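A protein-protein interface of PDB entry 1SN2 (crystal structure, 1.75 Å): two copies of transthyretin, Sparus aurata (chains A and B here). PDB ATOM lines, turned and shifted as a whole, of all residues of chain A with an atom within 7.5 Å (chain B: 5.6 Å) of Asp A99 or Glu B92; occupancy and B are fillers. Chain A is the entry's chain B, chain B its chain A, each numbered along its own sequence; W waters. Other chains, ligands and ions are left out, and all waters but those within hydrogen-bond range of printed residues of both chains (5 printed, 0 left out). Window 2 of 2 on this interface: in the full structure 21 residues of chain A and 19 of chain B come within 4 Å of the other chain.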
ATOM      1  N   LYS A  38      33.834  -2.486  20.003  1.00  0.00           N
ATOM      2  CA  LYS A  38      34.154  -1.995  18.670  1.00  0.00           C
ATOM      3  C   LYS A  38      35.560  -1.382  18.658  1.00  0.00           C
ATOM      4  O   LYS A  38      35.918  -0.645  19.570  1.00  0.00           O
ATOM      5  CB  LYS A  38      33.099  -0.974  18.242  1.00  0.00           C
ATOM      6  CG  LYS A  38      33.090  -0.696  16.747  1.00  0.00           C
ATOM      7  CD  LYS A  38      31.758  -0.134  16.242  1.00  0.00           C
ATOM      8  CE  LYS A  38      31.874   0.249  14.771  1.00  0.00           C
ATOM      9  NZ  LYS A  38      30.560   0.537  14.107  1.00  0.00           N
ATOM     10  N   TRP A  44      35.795  -5.712  15.766  1.00  0.00           N
ATOM     11  CA  TRP A  44      35.341  -6.081  17.101  1.00  0.00           C
ATOM     12  C   TRP A  44      36.408  -6.881  17.834  1.00  0.00           C
ATOM     13  O   TRP A  44      37.106  -7.690  17.225  1.00  0.00           O
ATOM     14  CB  TRP A  44      34.093  -6.951  16.997  1.00  0.00           C
ATOM     15  CG  TRP A  44      32.953  -6.253  16.359  1.00  0.00           C
ATOM     16  CD1 TRP A  44      32.550  -6.358  15.065  1.00  0.00           C
ATOM     17  CD2 TRP A  44      32.064  -5.328  16.987  1.00  0.00           C
ATOM     18  NE1 TRP A  44      31.458  -5.554  14.843  1.00  0.00           N
ATOM     19  CE2 TRP A  44      31.135  -4.913  16.015  1.00  0.00           C
ATOM     20  CE3 TRP A  44      31.941  -4.821  18.289  1.00  0.00           C
ATOM     21  CZ2 TRP A  44      30.118  -3.996  16.292  1.00  0.00           C
ATOM     22  CZ3 TRP A  44      30.935  -3.912  18.560  1.00  0.00           C
ATOM     23  CH2 TRP A  44      30.035  -3.511  17.569  1.00  0.00           C
ATOM     24  N   PHE A  67      35.734  -1.506  30.909  1.00  0.00           N
ATOM     25  CA  PHE A  67      34.513  -0.938  30.305  1.00  0.00           C
ATOM     26  C   PHE A  67      34.583   0.591  30.113  1.00  0.00           C
ATOM     27  O   PHE A  67      33.785   1.338  30.677  1.00  0.00           O
ATOM     28  CB  PHE A  67      33.292  -1.323  31.173  1.00  0.00           C
ATOM     29  CG  PHE A  67      31.943  -1.172  30.484  1.00  0.00           C
ATOM     30  CD1 PHE A  67      31.624  -1.917  29.359  1.00  0.00           C
ATOM     31  CD2 PHE A  67      30.978  -0.325  31.007  1.00  0.00           C
ATOM     32  CE1 PHE A  67      30.386  -1.788  28.747  1.00  0.00           C
ATOM     33  CE2 PHE A  67      29.736  -0.193  30.405  1.00  0.00           C
ATOM     34  CZ  PHE A  67      29.439  -0.927  29.276  1.00  0.00           C
ATOM     35  N   PRO A  68      35.526   1.070  29.319  1.00  0.00           N
ATOM     36  CA  PRO A  68      35.581   2.505  29.040  1.00  0.00           C
ATOM     37  C   PRO A  68      34.512   2.858  28.027  1.00  0.00           C
ATOM     38  O   PRO A  68      33.951   1.961  27.408  1.00  0.00           O
ATOM     39  CB  PRO A  68      36.956   2.667  28.399  1.00  0.00           C
ATOM     40  CG  PRO A  68      37.139   1.380  27.675  1.00  0.00           C
ATOM     41  CD  PRO A  68      36.624   0.352  28.649  1.00  0.00           C
ATOM     42  N   ALA A  69      34.225   4.145  27.863  1.00  0.00           N
ATOM     43  CA  ALA A  69      33.283   4.585  26.848  1.00  0.00           C
ATOM     44  C   ALA A  69      33.664   4.022  25.476  1.00  0.00           C
ATOM     45  O   ALA A  69      34.838   3.980  25.089  1.00  0.00           O
ATOM     46  CB  ALA A  69      33.243   6.110  26.789  1.00  0.00           C
ATOM     47  N   GLY A  70      32.649   3.620  24.729  1.00  0.00           N
ATOM     48  CA  GLY A  70      32.845   3.102  23.392  1.00  0.00           C
ATOM     49  C   GLY A  70      31.646   2.271  23.005  1.00  0.00           C
ATOM     50  O   GLY A  70      30.725   2.102  23.800  1.00  0.00           O
ATOM     51  N   VAL A  71      31.673   1.728  21.795  1.00  0.00           N
ATOM     52  CA  VAL A  71      30.593   0.876  21.317  1.00  0.00           C
ATOM     53  C   VAL A  71      30.842  -0.584  21.680  1.00  0.00           C
ATOM     54  O   VAL A  71      31.936  -1.111  21.485  1.00  0.00           O
ATOM     55  CB  VAL A  71      30.400   1.033  19.805  1.00  0.00           C
ATOM     56  CG1 VAL A  71      29.410   0.010  19.282  1.00  0.00           C
ATOM     57  CG2 VAL A  71      29.928   2.450  19.496  1.00  0.00           C
ATOM     58  N   TYR A  72      29.804  -1.219  22.217  1.00  0.00           N
ATOM     59  CA  TYR A  72      29.839  -2.612  22.613  1.00  0.00           C
ATOM     60  C   TYR A  72      28.716  -3.373  21.936  1.00  0.00           C
ATOM     61  O   TYR A  72      27.672  -2.809  21.581  1.00  0.00           O
ATOM     62  CB  TYR A  72      29.705  -2.758  24.123  1.00  0.00           C
ATOM     63  CG  TYR A  72      30.898  -2.207  24.861  1.00  0.00           C
ATOM     64  CD1 TYR A  72      31.011  -0.843  25.105  1.00  0.00           C
ATOM     65  CD2 TYR A  72      31.931  -3.038  25.271  1.00  0.00           C
ATOM     66  CE1 TYR A  72      32.122  -0.327  25.765  1.00  0.00           C
ATOM     67  CE2 TYR A  72      33.048  -2.535  25.943  1.00  0.00           C
ATOM     68  CZ  TYR A  72      33.137  -1.177  26.182  1.00  0.00           C
ATOM     69  OH  TYR A  72      34.242  -0.659  26.835  1.00  0.00           O
ATOM     70  N   VAL A  96      22.661  -6.854  20.910  1.00  0.00           N
ATOM     71  CA  VAL A  96      22.391  -5.547  21.497  1.00  0.00           C
ATOM     72  C   VAL A  96      23.653  -4.735  21.318  1.00  0.00           C
ATOM     73  O   VAL A  96      24.687  -5.049  21.912  1.00  0.00           O
ATOM     74  CB  VAL A  96      22.036  -5.666  22.976  1.00  0.00           C
ATOM     75  CG1 VAL A  96      21.765  -4.291  23.604  1.00  0.00           C
ATOM     76  CG2 VAL A  96      20.837  -6.576  23.139  1.00  0.00           C
ATOM     77  N   VAL A  97      23.559  -3.686  20.513  1.00  0.00           N
ATOM     78  CA  VAL A  97      24.708  -2.860  20.169  1.00  0.00           C
ATOM     79  C   VAL A  97      24.447  -1.451  20.671  1.00  0.00           C
ATOM     80  O   VAL A  97      23.434  -0.854  20.325  1.00  0.00           O
ATOM     81  CB  VAL A  97      24.919  -2.832  18.665  1.00  0.00           C
ATOM     82  CG1 VAL A  97      26.217  -2.130  18.338  1.00  0.00           C
ATOM     83  CG2 VAL A  97      24.907  -4.250  18.097  1.00  0.00           C
ATOM     84  N   PHE A  98      25.362  -0.931  21.475  1.00  0.00           N
ATOM     85  CA  PHE A  98      25.179   0.371  22.117  1.00  0.00           C
ATOM     86  C   PHE A  98      26.496   1.094  22.414  1.00  0.00           C
ATOM     87  O   PHE A  98      27.527   0.457  22.646  1.00  0.00           O
ATOM     88  CB  PHE A  98      24.397   0.167  23.418  1.00  0.00           C
ATOM     89  CG  PHE A  98      25.139  -0.623  24.476  1.00  0.00           C
ATOM     90  CD1 PHE A  98      25.705   0.022  25.565  1.00  0.00           C
ATOM     91  CD2 PHE A  98      25.254  -1.994  24.392  1.00  0.00           C
ATOM     92  CE1 PHE A  98      26.369  -0.692  26.556  1.00  0.00           C
ATOM     93  CE2 PHE A  98      25.937  -2.710  25.383  1.00  0.00           C
ATOM     94  CZ  PHE A  98      26.488  -2.047  26.457  1.00  0.00           C
ATOM     95  N   ASP A  99      26.463   2.423  22.405  1.00  0.00           N
ATOM     96  CA  ASP A  99      27.624   3.215  22.827  1.00  0.00           C
ATOM     97  C   ASP A  99      27.539   3.381  24.339  1.00  0.00           C
ATOM     98  O   ASP A  99      26.621   4.023  24.836  1.00  0.00           O
ATOM     99  CB  ASP A  99      27.623   4.588  22.164  1.00  0.00           C
ATOM    100  CG  ASP A  99      28.965   5.302  22.273  1.00  0.00           C
ATOM    101  OD1 ASP A  99      28.998   6.526  22.023  1.00  0.00           O
ATOM    102  OD2 ASP A  99      30.038   4.745  22.592  1.00  0.00           O
ATOM    103  N   ALA A 100      28.488   2.811  25.071  1.00  0.00           N
ATOM    104  CA  ALA A 100      28.468   2.888  26.528  1.00  0.00           C
ATOM    105  C   ALA A 100      29.101   4.187  27.026  1.00  0.00           C
ATOM    106  O   ALA A 100      30.141   4.604  26.535  1.00  0.00           O
ATOM    107  CB  ALA A 100      29.193   1.706  27.117  1.00  0.00           C
ATOM    108  N   HIS A 101      28.444   4.824  27.994  1.00  0.00           N
ATOM    109  CA  HIS A 101      28.945   6.035  28.643  1.00  0.00           C
ATOM    110  C   HIS A 101      28.883   5.797  30.148  1.00  0.00           C
ATOM    111  O   HIS A 101      27.900   6.121  30.814  1.00  0.00           O
ATOM    112  CB  HIS A 101      28.087   7.226  28.264  1.00  0.00           C
ATOM    113  CG  HIS A 101      27.850   7.338  26.796  1.00  0.00           C
ATOM    114  ND1 HIS A 101      26.586   7.345  26.250  1.00  0.00           N
ATOM    115  CD2 HIS A 101      28.712   7.432  25.757  1.00  0.00           C
ATOM    116  CE1 HIS A 101      26.682   7.439  24.937  1.00  0.00           C
ATOM    117  NE2 HIS A 101      27.958   7.489  24.612  1.00  0.00           N
ATOM    118  N   PRO A 102      29.911   5.177  30.688  1.00  0.00           N
ATOM    119  CA  PRO A 102      29.897   4.809  32.096  1.00  0.00           C
ATOM    120  C   PRO A 102      30.466   5.869  32.994  1.00  0.00           C
ATOM    121  O   PRO A 102      30.554   5.627  34.191  1.00  0.00           O
ATOM    122  CB  PRO A 102      30.826   3.621  32.111  1.00  0.00           C
ATOM    123  CG  PRO A 102      31.887   4.098  31.249  1.00  0.00           C
ATOM    124  CD  PRO A 102      31.148   4.713  30.044  1.00  0.00           C
ATOM    125  N   TYR A 108      25.170  -0.331  33.482  1.00  0.00           N
ATOM    126  CA  TYR A 108      24.157  -0.747  32.531  1.00  0.00           C
ATOM    127  C   TYR A 108      23.604  -2.109  32.849  1.00  0.00           C
ATOM    128  O   TYR A 108      24.353  -3.028  33.165  1.00  0.00           O
ATOM    129  CB  TYR A 108      24.781  -0.850  31.139  1.00  0.00           C
ATOM    130  CG  TYR A 108      25.088   0.490  30.536  1.00  0.00           C
ATOM    131  CD1 TYR A 108      26.226   1.190  30.883  1.00  0.00           C
ATOM    132  CD2 TYR A 108      24.226   1.053  29.620  1.00  0.00           C
ATOM    133  CE1 TYR A 108      26.483   2.419  30.334  1.00  0.00           C
ATOM    134  CE2 TYR A 108      24.474   2.271  29.068  1.00  0.00           C
ATOM    135  CZ  TYR A 108      25.599   2.958  29.428  1.00  0.00           C
ATOM    136  OH  TYR A 108      25.817   4.183  28.858  1.00  0.00           O
ATOM    137  N   PHE B  76      18.707  -1.566  11.143  1.00  0.00           N
ATOM    138  CA  PHE B  76      17.887  -0.375  11.128  1.00  0.00           C
ATOM    139  C   PHE B  76      18.625   0.751  11.850  1.00  0.00           C
ATOM    140  O   PHE B  76      19.096   0.553  12.976  1.00  0.00           O
ATOM    141  CB  PHE B  76      16.564  -0.619  11.875  1.00  0.00           C
ATOM    142  CG  PHE B  76      15.727  -1.748  11.328  1.00  0.00           C
ATOM    143  CD1 PHE B  76      15.973  -3.062  11.691  1.00  0.00           C
ATOM    144  CD2 PHE B  76      14.657  -1.484  10.501  1.00  0.00           C
ATOM    145  CE1 PHE B  76      15.180  -4.088  11.205  1.00  0.00           C
ATOM    146  CE2 PHE B  76      13.866  -2.496  10.023  1.00  0.00           C
ATOM    147  CZ  PHE B  76      14.131  -3.807  10.377  1.00  0.00           C
ATOM    148  N   ASP B  77      18.700   1.924  11.221  1.00  0.00           N
ATOM    149  CA  ASP B  77      19.398   3.067  11.801  1.00  0.00           C
ATOM    150  C   ASP B  77      18.484   3.798  12.775  1.00  0.00           C
ATOM    151  O   ASP B  77      18.040   4.926  12.534  1.00  0.00           O
ATOM    152  CB  ASP B  77      19.902   4.007  10.726  1.00  0.00           C
ATOM    153  CG  ASP B  77      20.851   5.051  11.263  1.00  0.00           C
ATOM    154  OD1 ASP B  77      21.053   5.128  12.504  1.00  0.00           O
ATOM    155  OD2 ASP B  77      21.450   5.845  10.507  1.00  0.00           O
ATOM    156  N   THR B  78      18.223   3.136  13.897  1.00  0.00           N
ATOM    157  CA  THR B  78      17.349   3.694  14.925  1.00  0.00           C
ATOM    158  C   THR B  78      18.001   4.872  15.652  1.00  0.00           C
ATOM    159  O   THR B  78      17.313   5.749  16.161  1.00  0.00           O
ATOM    160  CB  THR B  78      16.947   2.614  15.947  1.00  0.00           C
ATOM    161  OG1 THR B  78      18.103   1.995  16.518  1.00  0.00           O
ATOM    162  CG2 THR B  78      16.224   1.463  15.270  1.00  0.00           C
ATOM    163  N   LYS B  79      19.328   4.884  15.713  1.00  0.00           N
ATOM    164  CA  LYS B  79      20.007   5.951  16.436  1.00  0.00           C
ATOM    165  C   LYS B  79      19.756   7.279  15.728  1.00  0.00           C
ATOM    166  O   LYS B  79      19.474   8.299  16.377  1.00  0.00           O
ATOM    167  CB  LYS B  79      21.501   5.661  16.585  1.00  0.00           C
ATOM    168  CG  LYS B  79      22.240   6.720  17.403  1.00  0.00           C
ATOM    169  CD  LYS B  79      23.735   6.471  17.379  1.00  0.00           C
ATOM    170  CE  LYS B  79      24.495   7.392  18.313  1.00  0.00           C
ATOM    171  NZ  LYS B  79      25.977   7.138  18.247  1.00  0.00           N
ATOM    172  N   PHE B  90      19.383   4.730  23.142  1.00  0.00           N
ATOM    173  CA  PHE B  90      20.320   3.810  23.729  1.00  0.00           C
ATOM    174  C   PHE B  90      21.086   3.031  22.650  1.00  0.00           C
ATOM    175  O   PHE B  90      22.314   3.018  22.636  1.00  0.00           O
ATOM    176  CB  PHE B  90      19.614   2.819  24.646  1.00  0.00           C
ATOM    177  CG  PHE B  90      20.500   1.701  25.081  1.00  0.00           C
ATOM    178  CD1 PHE B  90      21.512   1.920  26.000  1.00  0.00           C
ATOM    179  CD2 PHE B  90      20.354   0.446  24.535  1.00  0.00           C
ATOM    180  CE1 PHE B  90      22.351   0.882  26.379  1.00  0.00           C
ATOM    181  CE2 PHE B  90      21.191  -0.586  24.905  1.00  0.00           C
ATOM    182  CZ  PHE B  90      22.189  -0.368  25.831  1.00  0.00           C
ATOM    183  N   HIS B  91      20.364   2.370  21.753  1.00  0.00           N
ATOM    184  CA  HIS B  91      21.004   1.478  20.788  1.00  0.00           C
ATOM    185  C   HIS B  91      21.715   2.220  19.668  1.00  0.00           C
ATOM    186  O   HIS B  91      21.275   3.294  19.221  1.00  0.00           O
ATOM    187  CB  HIS B  91      19.975   0.531  20.170  1.00  0.00           C
ATOM    188  CG  HIS B  91      19.269  -0.338  21.161  1.00  0.00           C
ATOM    189  ND1 HIS B  91      18.065   0.015  21.737  1.00  0.00           N
ATOM    190  CD2 HIS B  91      19.562  -1.577  21.628  1.00  0.00           C
ATOM    191  CE1 HIS B  91      17.662  -0.959  22.534  1.00  0.00           C
ATOM    192  NE2 HIS B  91      18.548  -1.937  22.486  1.00  0.00           N
ATOM    193  N   GLU B  92      22.831   1.656  19.229  1.00  0.00           N
ATOM    194  CA  GLU B  92      23.576   2.212  18.093  1.00  0.00           C
ATOM    195  C   GLU B  92      22.845   1.894  16.813  1.00  0.00           C
ATOM    196  O   GLU B  92      22.890   2.660  15.850  1.00  0.00           O
ATOM    197  CB  GLU B  92      24.967   1.599  17.984  1.00  0.00           C
ATOM    198  CG  GLU B  92      26.057   2.265  18.780  1.00  0.00           C
ATOM    199  CD  GLU B  92      26.288   3.713  18.392  1.00  0.00           C
ATOM    200  OE1 GLU B  92      27.038   3.993  17.433  1.00  0.00           O
ATOM    201  OE2 GLU B  92      25.723   4.571  19.066  1.00  0.00           O
ATOM    202  N   VAL B  93      22.207   0.729  16.802  1.00  0.00           N
ATOM    203  CA  VAL B  93      21.471   0.233  15.666  1.00  0.00           C
ATOM    204  C   VAL B  93      20.534  -0.846  16.186  1.00  0.00           C
ATOM    205  O   VAL B  93      20.743  -1.360  17.289  1.00  0.00           O
ATOM    206  CB  VAL B  93      22.453  -0.401  14.649  1.00  0.00           C
ATOM    207  CG1 VAL B  93      23.256  -1.510  15.295  1.00  0.00           C
ATOM    208  CG2 VAL B  93      21.656  -0.946  13.463  1.00  0.00           C
ATOM    209  N   ALA B  94      19.481  -1.160  15.437  1.00  0.00           N
ATOM    210  CA  ALA B  94      18.654  -2.305  15.778  1.00  0.00           C
ATOM    211  C   ALA B  94      18.974  -3.380  14.747  1.00  0.00           C
ATOM    212  O   ALA B  94      18.882  -3.136  13.544  1.00  0.00           O
ATOM    213  CB  ALA B  94      17.209  -1.961  15.747  1.00  0.00           C
HETATM  214  O   HOH W   1      28.963   3.103  15.650  1.00  0.00           O
HETATM  215  O   HOH W   2      23.933   4.326  24.620  1.00  0.00           O
HETATM  216  O   HOH W   3      24.450   4.057  21.230  1.00  0.00           O
HETATM  217  O   HOH W   4      21.060  -3.355  19.084  1.00  0.00           O
HETATM  218  O   HOH W   5      26.839   7.919  21.083  1.00  0.00           O
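The backbone carbonyl oxygen of Val A97 sits at hydrogen-bond distance from the backbone NH of Glu B92, at 2.8 Å.
NZ of Lys B79 is in salt-bridge range of OE2 of Glu B92 (2.7 Å). O of Val A71 lies within hydrogen-bond range of N of Lys A38, at 2.8 Å. N of Tyr A72 lies within hydrogen-bond range of O of Phe A98 (2.9 Å). The side-chain carboxylate (OD1) of Asp A99 sits at hydrogen-bond distance from a ring nitrogen (NE2) of His A101 (3.0 Å). The side-chain hydroxyl (OH) of Tyr A108 lies within hydrogen-bond range of the backbone NH (N) of His A101 (2.8 Å).
Among the printed residues, pairs that only touch across the chains: Phe A98 with Phe B90 (3.3 Å), Val A97 with His B91 (3.4 Å), Asp A99 with Glu B92 (3.6 Å), Tyr A108 with Phe B90 (3.7 Å), Phe A98 with Glu B92 (3.8 Å), Val A71 with Glu B92 (3.9 Å), Val A96 with Phe B90 (3.97 Å) and Val A97 with Val B93 (3.98 Å).
Of chain B, only Glu B92 (3.6 Å) comes within 4 Å of Asp A99. Glu B92 touches just these residues of chain A: Val A71 (3.9 Å), Val A97 (2.8 Å), Phe A98 (3.8 Å) and Asp A99 (3.6 Å). Printed residues of chain B within 4 Å of Val A97: His B91, Glu B92 and Val B93. Printed residues of chain B within 4 Å of Val A96: Phe B90 (3.97 Å). Printed residues of chain B within 4 Å of Tyr A108: Phe B90 (3.7 Å). Of the printed residues of chain B, Phe A98 touches Phe B90 (3.3 Å) and Glu B92 (3.8 Å). Printed residues of chain A within 4 Å of Val B93: Val A97 (3.98 Å). Thr B78 touches none of the printed residues of chain A. Pro A102 touches none of the printed residues of chain B. The nearest residue of chain B that does not touch Asp A99 is Phe B90 (4.2 Å).
Hydrophobic or aromatic side chains of chain A within 4 Å of the printed part of chain B: Val A71, Val A96, Val A97, Phe A98 and Tyr A108. Of the 9 printed residues of chain B, 4 touch a printed residue of chain A. Printed residues of chain B that touch a printed residue of chain A: Phe B90, His B91, Glu B92 and Val B93. Among the printed residues, 9 pairs touch across the chains. Among the printed residues, no Asp or Glu carboxylate lies within 4 Å of a Lys or Arg side-chain nitrogen of the other chain.
No position is printed for both chains. Of the 9 pairs that touch across the chains among the printed residues, none has its exchanged pair printed and touching as well.
Water W3 lies within hydrogen-bond range of the side-chain carboxylate (OE2) of Glu B92 (2.6 Å), the backbone carbonyl oxygen (O) of Phe B90 (2.8 Å) and the backbone NH (N) of Asp A99 (2.8 Å). Water W4 bridges the backbone carbonyl oxygen (O) of Val B93 (2.7 Å) and the backbone NH (N) of Val A97 (2.9 Å). Water W2 bridges O of Asp A99 (2.7 Å) and O of Phe B90 (2.9 Å). Water W5 lies within hydrogen-bond range of the side-chain carboxylate (OD1) of Asp A99 (2.7 Å) and the side-chain amino group (NZ) of Lys B79 (3.1 Å). Water W1 bridges OE1 of Glu B92 (2.8 Å) and NZ of Lys A38 (3.4 Å).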
